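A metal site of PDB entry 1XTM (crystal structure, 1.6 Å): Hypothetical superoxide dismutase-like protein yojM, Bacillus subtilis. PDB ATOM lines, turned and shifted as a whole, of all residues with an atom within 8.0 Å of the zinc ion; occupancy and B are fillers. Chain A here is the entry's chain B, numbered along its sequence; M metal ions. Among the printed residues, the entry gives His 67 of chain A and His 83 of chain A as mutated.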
ATOM      1  N   PHE A  64      34.120  24.736  29.963  1.00  0.00           N
ATOM      2  CA  PHE A  64      33.898  26.107  29.609  1.00  0.00           C
ATOM      3  C   PHE A  64      32.603  26.209  28.812  1.00  0.00           C
ATOM      4  O   PHE A  64      32.481  25.606  27.737  1.00  0.00           O
ATOM      5  CB  PHE A  64      35.040  26.605  28.732  1.00  0.00           C
ATOM      6  CG  PHE A  64      34.949  28.079  28.380  1.00  0.00           C
ATOM      7  CD1 PHE A  64      34.533  29.045  29.349  1.00  0.00           C
ATOM      8  CD2 PHE A  64      35.421  28.534  27.118  1.00  0.00           C
ATOM      9  CE1 PHE A  64      34.504  30.404  29.003  1.00  0.00           C
ATOM     10  CE2 PHE A  64      35.412  29.908  26.792  1.00  0.00           C
ATOM     11  CZ  PHE A  64      34.957  30.846  27.743  1.00  0.00           C
ATOM     12  N   HIS A  65      31.655  26.980  29.346  1.00  0.00           N
ATOM     13  CA  HIS A  65      30.284  27.027  28.797  1.00  0.00           C
ATOM     14  C   HIS A  65      29.680  28.385  28.913  1.00  0.00           C
ATOM     15  O   HIS A  65      29.942  29.115  29.929  1.00  0.00           O
ATOM     16  CB  HIS A  65      29.289  26.097  29.546  1.00  0.00           C
ATOM     17  CG  HIS A  65      29.848  24.749  29.907  1.00  0.00           C
ATOM     18  ND1 HIS A  65      29.780  24.244  31.187  1.00  0.00           N
ATOM     19  CD2 HIS A  65      30.423  23.776  29.149  1.00  0.00           C
ATOM     20  CE1 HIS A  65      30.324  23.039  31.213  1.00  0.00           C
ATOM     21  NE2 HIS A  65      30.720  22.730  29.995  1.00  0.00           N
ATOM     22  N   ILE A  66      28.814  28.706  27.963  1.00  0.00           N
ATOM     23  CA  ILE A  66      27.952  29.866  28.107  1.00  0.00           C
ATOM     24  C   ILE A  66      26.682  29.398  28.797  1.00  0.00           C
ATOM     25  O   ILE A  66      25.979  28.452  28.340  1.00  0.00           O
ATOM     26  CB  ILE A  66      27.607  30.568  26.753  1.00  0.00           C
ATOM     27  CG1 ILE A  66      28.888  30.954  26.009  1.00  0.00           C
ATOM     28  CG2 ILE A  66      26.753  31.817  27.022  1.00  0.00           C
ATOM     29  CD1 ILE A  66      28.674  31.395  24.535  1.00  0.00           C
ATOM     30  N   HIS A  67      26.392  30.028  29.939  1.00  0.00           N
ATOM     31  CA  HIS A  67      25.192  29.714  30.721  1.00  0.00           C
ATOM     32  C   HIS A  67      24.061  30.749  30.430  1.00  0.00           C
ATOM     33  O   HIS A  67      24.329  31.861  29.939  1.00  0.00           O
ATOM     34  CB  HIS A  67      25.530  29.664  32.223  1.00  0.00           C
ATOM     35  CG  HIS A  67      26.291  28.433  32.618  1.00  0.00           C
ATOM     36  ND1 HIS A  67      25.788  27.513  33.519  1.00  0.00           N
ATOM     37  CD2 HIS A  67      27.471  27.928  32.194  1.00  0.00           C
ATOM     38  CE1 HIS A  67      26.654  26.528  33.679  1.00  0.00           C
ATOM     39  NE2 HIS A  67      27.685  26.761  32.881  1.00  0.00           N
ATOM     40  N   GLY A  82      21.420  27.445  33.566  1.00  0.00           N
ATOM     41  CA  GLY A  82      21.682  26.070  33.158  1.00  0.00           C
ATOM     42  C   GLY A  82      22.564  26.443  31.912  1.00  0.00           C
ATOM     43  O   GLY A  82      22.773  27.632  31.653  1.00  0.00           O
ATOM     44  N   HIS A  83      23.101  25.491  31.140  1.00  0.00           N
ATOM     45  CA  HIS A  83      23.816  25.822  29.896  1.00  0.00           C
ATOM     46  C   HIS A  83      22.834  26.459  28.883  1.00  0.00           C
ATOM     47  O   HIS A  83      21.656  26.063  28.850  1.00  0.00           O
ATOM     48  CB  HIS A  83      24.384  24.561  29.225  1.00  0.00           C
ATOM     49  CG  HIS A  83      25.472  23.877  29.982  1.00  0.00           C
ATOM     50  ND1 HIS A  83      26.183  22.801  29.474  1.00  0.00           N
ATOM     51  CD2 HIS A  83      25.996  24.125  31.214  1.00  0.00           C
ATOM     52  CE1 HIS A  83      27.085  22.414  30.363  1.00  0.00           C
ATOM     53  NE2 HIS A  83      27.003  23.203  31.412  1.00  0.00           N
ATOM     54  N   PHE A  84      23.299  27.412  28.092  1.00  0.00           N
ATOM     55  CA  PHE A  84      22.453  28.147  27.140  1.00  0.00           C
ATOM     56  C   PHE A  84      22.049  27.100  26.097  1.00  0.00           C
ATOM     57  O   PHE A  84      22.927  26.468  25.492  1.00  0.00           O
ATOM     58  CB  PHE A  84      23.252  29.281  26.505  1.00  0.00           C
ATOM     59  CG  PHE A  84      22.539  30.008  25.386  1.00  0.00           C
ATOM     60  CD1 PHE A  84      23.153  30.147  24.127  1.00  0.00           C
ATOM     61  CD2 PHE A  84      21.315  30.622  25.596  1.00  0.00           C
ATOM     62  CE1 PHE A  84      22.517  30.860  23.084  1.00  0.00           C
ATOM     63  CE2 PHE A  84      20.675  31.331  24.545  1.00  0.00           C
ATOM     64  CZ  PHE A  84      21.306  31.446  23.288  1.00  0.00           C
ATOM     65  N   ASN A  85      20.742  26.909  25.946  1.00  0.00           N
ATOM     66  CA  ASN A  85      20.184  25.744  25.180  1.00  0.00           C
ATOM     67  C   ASN A  85      18.885  26.088  24.414  1.00  0.00           C
ATOM     68  O   ASN A  85      17.820  25.441  24.643  1.00  0.00           O
ATOM     69  CB  ASN A  85      19.929  24.600  26.174  1.00  0.00           C
ATOM     70  CG  ASN A  85      19.650  23.245  25.495  1.00  0.00           C
ATOM     71  OD1 ASN A  85      20.001  23.018  24.323  1.00  0.00           O
ATOM     72  ND2 ASN A  85      19.040  22.347  26.249  1.00  0.00           N
ATOM     73  N   LYS A  89      18.665  20.722  23.105  1.00  0.00           N
ATOM     74  CA  LYS A  89      19.469  19.499  22.979  1.00  0.00           C
ATOM     75  C   LYS A  89      20.054  19.034  24.334  1.00  0.00           C
ATOM     76  O   LYS A  89      19.904  19.726  25.360  1.00  0.00           O
ATOM     77  CB  LYS A  89      20.575  19.690  21.926  1.00  0.00           C
ATOM     78  CG  LYS A  89      20.177  20.565  20.738  1.00  0.00           C
ATOM     79  CD  LYS A  89      21.032  20.362  19.518  1.00  0.00           C
ATOM     80  CE  LYS A  89      20.363  19.415  18.501  1.00  0.00           C
ATOM     81  NZ  LYS A  89      21.392  18.892  17.532  1.00  0.00           N
ATOM     82  N   GLU A  90      20.677  17.844  24.328  1.00  0.00           N
ATOM     83  CA  GLU A  90      21.416  17.308  25.473  1.00  0.00           C
ATOM     84  C   GLU A  90      22.807  17.895  25.469  1.00  0.00           C
ATOM     85  O   GLU A  90      23.192  18.597  24.524  1.00  0.00           O
ATOM     86  CB  GLU A  90      21.497  15.779  25.404  1.00  0.00           C
ATOM     87  CG  GLU A  90      20.176  15.056  25.656  1.00  0.00           C
ATOM     88  CD  GLU A  90      20.356  13.554  25.824  1.00  0.00           C
ATOM     89  OE1 GLU A  90      21.526  13.086  25.910  1.00  0.00           O
ATOM     90  OE2 GLU A  90      19.323  12.826  25.858  1.00  0.00           O
ATOM     91  N   HIS A  91      23.578  17.628  26.524  1.00  0.00           N
ATOM     92  CA  HIS A  91      24.942  18.126  26.557  1.00  0.00           C
ATOM     93  C   HIS A  91      25.925  17.325  25.688  1.00  0.00           C
ATOM     94  O   HIS A  91      25.883  16.103  25.656  1.00  0.00           O
ATOM     95  CB  HIS A  91      25.447  18.173  28.010  1.00  0.00           C
ATOM     96  CG  HIS A  91      26.856  18.649  28.125  1.00  0.00           C
ATOM     97  ND1 HIS A  91      27.204  19.993  27.997  1.00  0.00           N
ATOM     98  CD2 HIS A  91      28.020  17.976  28.276  1.00  0.00           C
ATOM     99  CE1 HIS A  91      28.516  20.107  28.071  1.00  0.00           C
ATOM    100  NE2 HIS A  91      29.040  18.903  28.259  1.00  0.00           N
ATOM    101  N   GLY A  92      26.853  18.023  25.030  1.00  0.00           N
ATOM    102  CA  GLY A  92      28.123  17.425  24.650  1.00  0.00           C
ATOM    103  C   GLY A  92      28.392  17.212  23.169  1.00  0.00           C
ATOM    104  O   GLY A  92      27.551  16.636  22.459  1.00  0.00           O
ATOM    105  N   PHE A  93      29.561  17.667  22.710  1.00  0.00           N
ATOM    106  CA  PHE A  93      29.958  17.523  21.293  1.00  0.00           C
ATOM    107  C   PHE A  93      29.967  16.069  20.848  1.00  0.00           C
ATOM    108  O   PHE A  93      29.760  15.823  19.654  1.00  0.00           O
ATOM    109  CB  PHE A  93      31.357  18.065  20.995  1.00  0.00           C
ATOM    110  CG  PHE A  93      31.529  19.533  21.301  1.00  0.00           C
ATOM    111  CD1 PHE A  93      32.585  19.948  22.093  1.00  0.00           C
ATOM    112  CD2 PHE A  93      30.644  20.476  20.813  1.00  0.00           C
ATOM    113  CE1 PHE A  93      32.755  21.306  22.398  1.00  0.00           C
ATOM    114  CE2 PHE A  93      30.825  21.839  21.098  1.00  0.00           C
ATOM    115  CZ  PHE A  93      31.883  22.245  21.905  1.00  0.00           C
ATOM    116  N   HIS A  99      24.156  19.143  20.734  1.00  0.00           N
ATOM    117  CA  HIS A  99      24.759  19.664  21.981  1.00  0.00           C
ATOM    118  C   HIS A  99      24.201  21.044  22.256  1.00  0.00           C
ATOM    119  O   HIS A  99      23.602  21.677  21.405  1.00  0.00           O
ATOM    120  CB  HIS A  99      26.289  19.754  21.879  1.00  0.00           C
ATOM    121  CG  HIS A  99      26.794  20.467  20.672  1.00  0.00           C
ATOM    122  ND1 HIS A  99      27.103  19.786  19.494  1.00  0.00           N
ATOM    123  CD2 HIS A  99      27.106  21.765  20.437  1.00  0.00           C
ATOM    124  CE1 HIS A  99      27.571  20.648  18.610  1.00  0.00           C
ATOM    125  NE2 HIS A  99      27.578  21.854  19.149  1.00  0.00           N
ATOM    126  N   HIS A 100      24.397  21.527  23.464  1.00  0.00           N
ATOM    127  CA  HIS A 100      23.970  22.876  23.760  1.00  0.00           C
ATOM    128  C   HIS A 100      24.682  23.937  22.961  1.00  0.00           C
ATOM    129  O   HIS A 100      25.897  23.850  22.751  1.00  0.00           O
ATOM    130  CB  HIS A 100      24.240  23.140  25.225  1.00  0.00           C
ATOM    131  CG  HIS A 100      23.584  22.153  26.144  1.00  0.00           C
ATOM    132  ND1 HIS A 100      24.175  21.686  27.296  1.00  0.00           N
ATOM    133  CD2 HIS A 100      22.365  21.583  26.096  1.00  0.00           C
ATOM    134  CE1 HIS A 100      23.349  20.860  27.911  1.00  0.00           C
ATOM    135  NE2 HIS A 100      22.244  20.783  27.204  1.00  0.00           N
ATOM    136  N   ALA A 101      23.913  24.945  22.592  1.00  0.00           N
ATOM    137  CA  ALA A 101      24.424  26.096  21.899  1.00  0.00           C
ATOM    138  C   ALA A 101      25.596  26.750  22.714  1.00  0.00           C
ATOM    139  O   ALA A 101      26.588  27.234  22.150  1.00  0.00           O
ATOM    140  CB  ALA A 101      23.309  27.074  21.658  1.00  0.00           C
ATOM    141  N   GLY A 102      25.459  26.625  24.012  1.00  0.00           N
ATOM    142  CA  GLY A 102      26.457  27.208  24.963  1.00  0.00           C
ATOM    143  C   GLY A 102      27.672  26.324  25.212  1.00  0.00           C
ATOM    144  O   GLY A 102      28.583  26.689  26.011  1.00  0.00           O
ATOM    145  N   ASP A 103      27.752  25.155  24.557  1.00  0.00           N
ATOM    146  CA  ASP A 103      28.875  24.245  24.812  1.00  0.00           C
ATOM    147  C   ASP A 103      30.075  24.721  24.070  1.00  0.00           C
ATOM    148  O   ASP A 103      30.004  24.894  22.851  1.00  0.00           O
ATOM    149  CB  ASP A 103      28.585  22.752  24.455  1.00  0.00           C
ATOM    150  CG  ASP A 103      27.575  22.132  25.391  1.00  0.00           C
ATOM    151  OD1 ASP A 103      27.048  21.018  25.108  1.00  0.00           O
ATOM    152  OD2 ASP A 103      27.216  22.685  26.468  1.00  0.00           O
ATOM    153  N   LEU A 104      31.183  24.911  24.800  1.00  0.00           N
ATOM    154  CA  LEU A 104      32.421  25.386  24.170  1.00  0.00           C
ATOM    155  C   LEU A 104      33.567  24.409  24.454  1.00  0.00           C
ATOM    156  O   LEU A 104      33.421  23.587  25.358  1.00  0.00           O
ATOM    157  CB  LEU A 104      32.801  26.763  24.721  1.00  0.00           C
ATOM    158  CG  LEU A 104      31.863  27.939  24.528  1.00  0.00           C
ATOM    159  CD1 LEU A 104      32.456  29.205  25.201  1.00  0.00           C
ATOM    160  CD2 LEU A 104      31.560  28.196  23.042  1.00  0.00           C
ATOM    161  N   ASP A 149      35.364  19.028  30.804  1.00  0.00           N
ATOM    162  CA  ASP A 149      34.102  18.602  30.232  1.00  0.00           C
ATOM    163  C   ASP A 149      34.405  17.325  29.375  1.00  0.00           C
ATOM    164  O   ASP A 149      35.316  17.352  28.541  1.00  0.00           O
ATOM    165  CB  ASP A 149      33.570  19.752  29.361  1.00  0.00           C
ATOM    166  CG  ASP A 149      32.136  19.529  28.858  1.00  0.00           C
ATOM    167  OD1 ASP A 149      31.713  18.351  28.683  1.00  0.00           O
ATOM    168  OD2 ASP A 149      31.388  20.503  28.623  1.00  0.00           O
ATOM    169  N   THR A 153      28.438  13.592  29.034  1.00  0.00           N
ATOM    170  CA  THR A 153      27.548  13.348  30.148  1.00  0.00           C
ATOM    171  C   THR A 153      26.611  14.523  30.356  1.00  0.00           C
ATOM    172  O   THR A 153      27.031  15.683  30.341  1.00  0.00           O
ATOM    173  CB  THR A 153      28.380  13.106  31.424  1.00  0.00           C
ATOM    174  OG1 THR A 153      29.213  11.958  31.230  1.00  0.00           O
ATOM    175  CG2 THR A 153      27.480  12.702  32.597  1.00  0.00           C
ATOM    176  N   ASN A 154      25.324  14.231  30.545  1.00  0.00           N
ATOM    177  CA  ASN A 154      24.373  15.234  30.985  1.00  0.00           C
ATOM    178  C   ASN A 154      24.492  15.554  32.462  1.00  0.00           C
ATOM    179  O   ASN A 154      24.891  14.695  33.265  1.00  0.00           O
ATOM    180  CB  ASN A 154      22.954  14.772  30.679  1.00  0.00           C
ATOM    181  CG  ASN A 154      22.602  14.938  29.219  1.00  0.00           C
ATOM    182  OD1 ASN A 154      22.420  16.057  28.726  1.00  0.00           O
ATOM    183  ND2 ASN A 154      22.492  13.817  28.516  1.00  0.00           N
ATOM    184  N   PRO A 155      24.130  16.796  32.830  1.00  0.00           N
ATOM    185  CA  PRO A 155      23.850  17.868  31.860  1.00  0.00           C
ATOM    186  C   PRO A 155      25.033  18.837  31.608  1.00  0.00           C
ATOM    187  O   PRO A 155      24.881  19.781  30.818  1.00  0.00           O
ATOM    188  CB  PRO A 155      22.682  18.598  32.528  1.00  0.00           C
ATOM    189  CG  PRO A 155      22.971  18.463  34.005  1.00  0.00           C
ATOM    190  CD  PRO A 155      23.851  17.225  34.216  1.00  0.00           C
ATOM    191  N   SER A 156      26.175  18.619  32.266  1.00  0.00           N
ATOM    192  CA  SER A 156      27.342  19.504  32.150  1.00  0.00           C
ATOM    193  C   SER A 156      28.694  18.825  31.870  1.00  0.00           C
ATOM    194  O   SER A 156      29.748  19.419  32.093  1.00  0.00           O
ATOM    195  CB  SER A 156      27.455  20.383  33.411  1.00  0.00           C
ATOM    196  OG  SER A 156      27.095  19.606  34.552  1.00  0.00           O
ATOM    197  N   GLY A 157      28.678  17.570  31.391  1.00  0.00           N
ATOM    198  CA  GLY A 157      29.905  16.871  31.037  1.00  0.00           C
ATOM    199  C   GLY A 157      30.783  16.505  32.213  1.00  0.00           C
ATOM    200  O   GLY A 157      31.971  16.259  32.057  1.00  0.00           O
ATOM    201  N   SER A 159      31.807  18.365  34.492  1.00  0.00           N
ATOM    202  CA  SER A 159      32.749  19.484  34.646  1.00  0.00           C
ATOM    203  C   SER A 159      32.944  19.916  36.112  1.00  0.00           C
ATOM    204  O   SER A 159      33.867  20.647  36.423  1.00  0.00           O
ATOM    205  CB  SER A 159      32.292  20.714  33.812  1.00  0.00           C
ATOM    206  OG  SER A 159      32.153  20.375  32.424  1.00  0.00           O
HETATM  207 ZN    ZN M   1      26.142  21.740  27.817  1.00  0.00          ZN
HETATM  208 CU    CU M   2      29.040  25.196  32.859  1.00  0.00          CU
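OD2 of Asp 103 is bound to the zinc ion (2.0 Å).
ND1 of His 83 binds the zinc ion, at 2.0 Å.
The zinc ion is bound by a ring nitrogen (ND1) of His 100 (2.0 Å).
ND1 of His 91 binds the zinc ion.
The zinc ion has four donor atoms within binding distance.
Pro 155 touches the zinc ion.
Five residues have an atom within 4 Å of the zinc ion: His 83, His 91, His 100, Asp 103 and Pro 155.
Along chain A the residues within 4 Å of the zinc ion span positions 83 to 155.
N of His 100 sits at hydrogen-bond distance from O of Glu 90, at 3.3 Å.
A ring nitrogen (NE2) of His 100 lies within hydrogen-bond range of the backbone carbonyl oxygen (O) of Lys 89, 3.2 Å away.
The backbone NH of His 91 sits at hydrogen-bond distance from the side-chain amide oxygen of Asn 154 (2.9 Å).
A ring nitrogen (NE2) of His 91 sits close to the backbone NH (N) of Gly 157 (3.4 Å).
A ring nitrogen (NE2) of His 83 lies close to a ring nitrogen (ND1) of His 65, at 3.0 Å.
NE2 of His 91 lies within hydrogen-bond range of OD1 of Asp 149, 2.8 Å away.
The backbone NH of Gly 92 is in hydrogen-bond range of the side-chain carboxylate of Asp 103 (3.0 Å).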
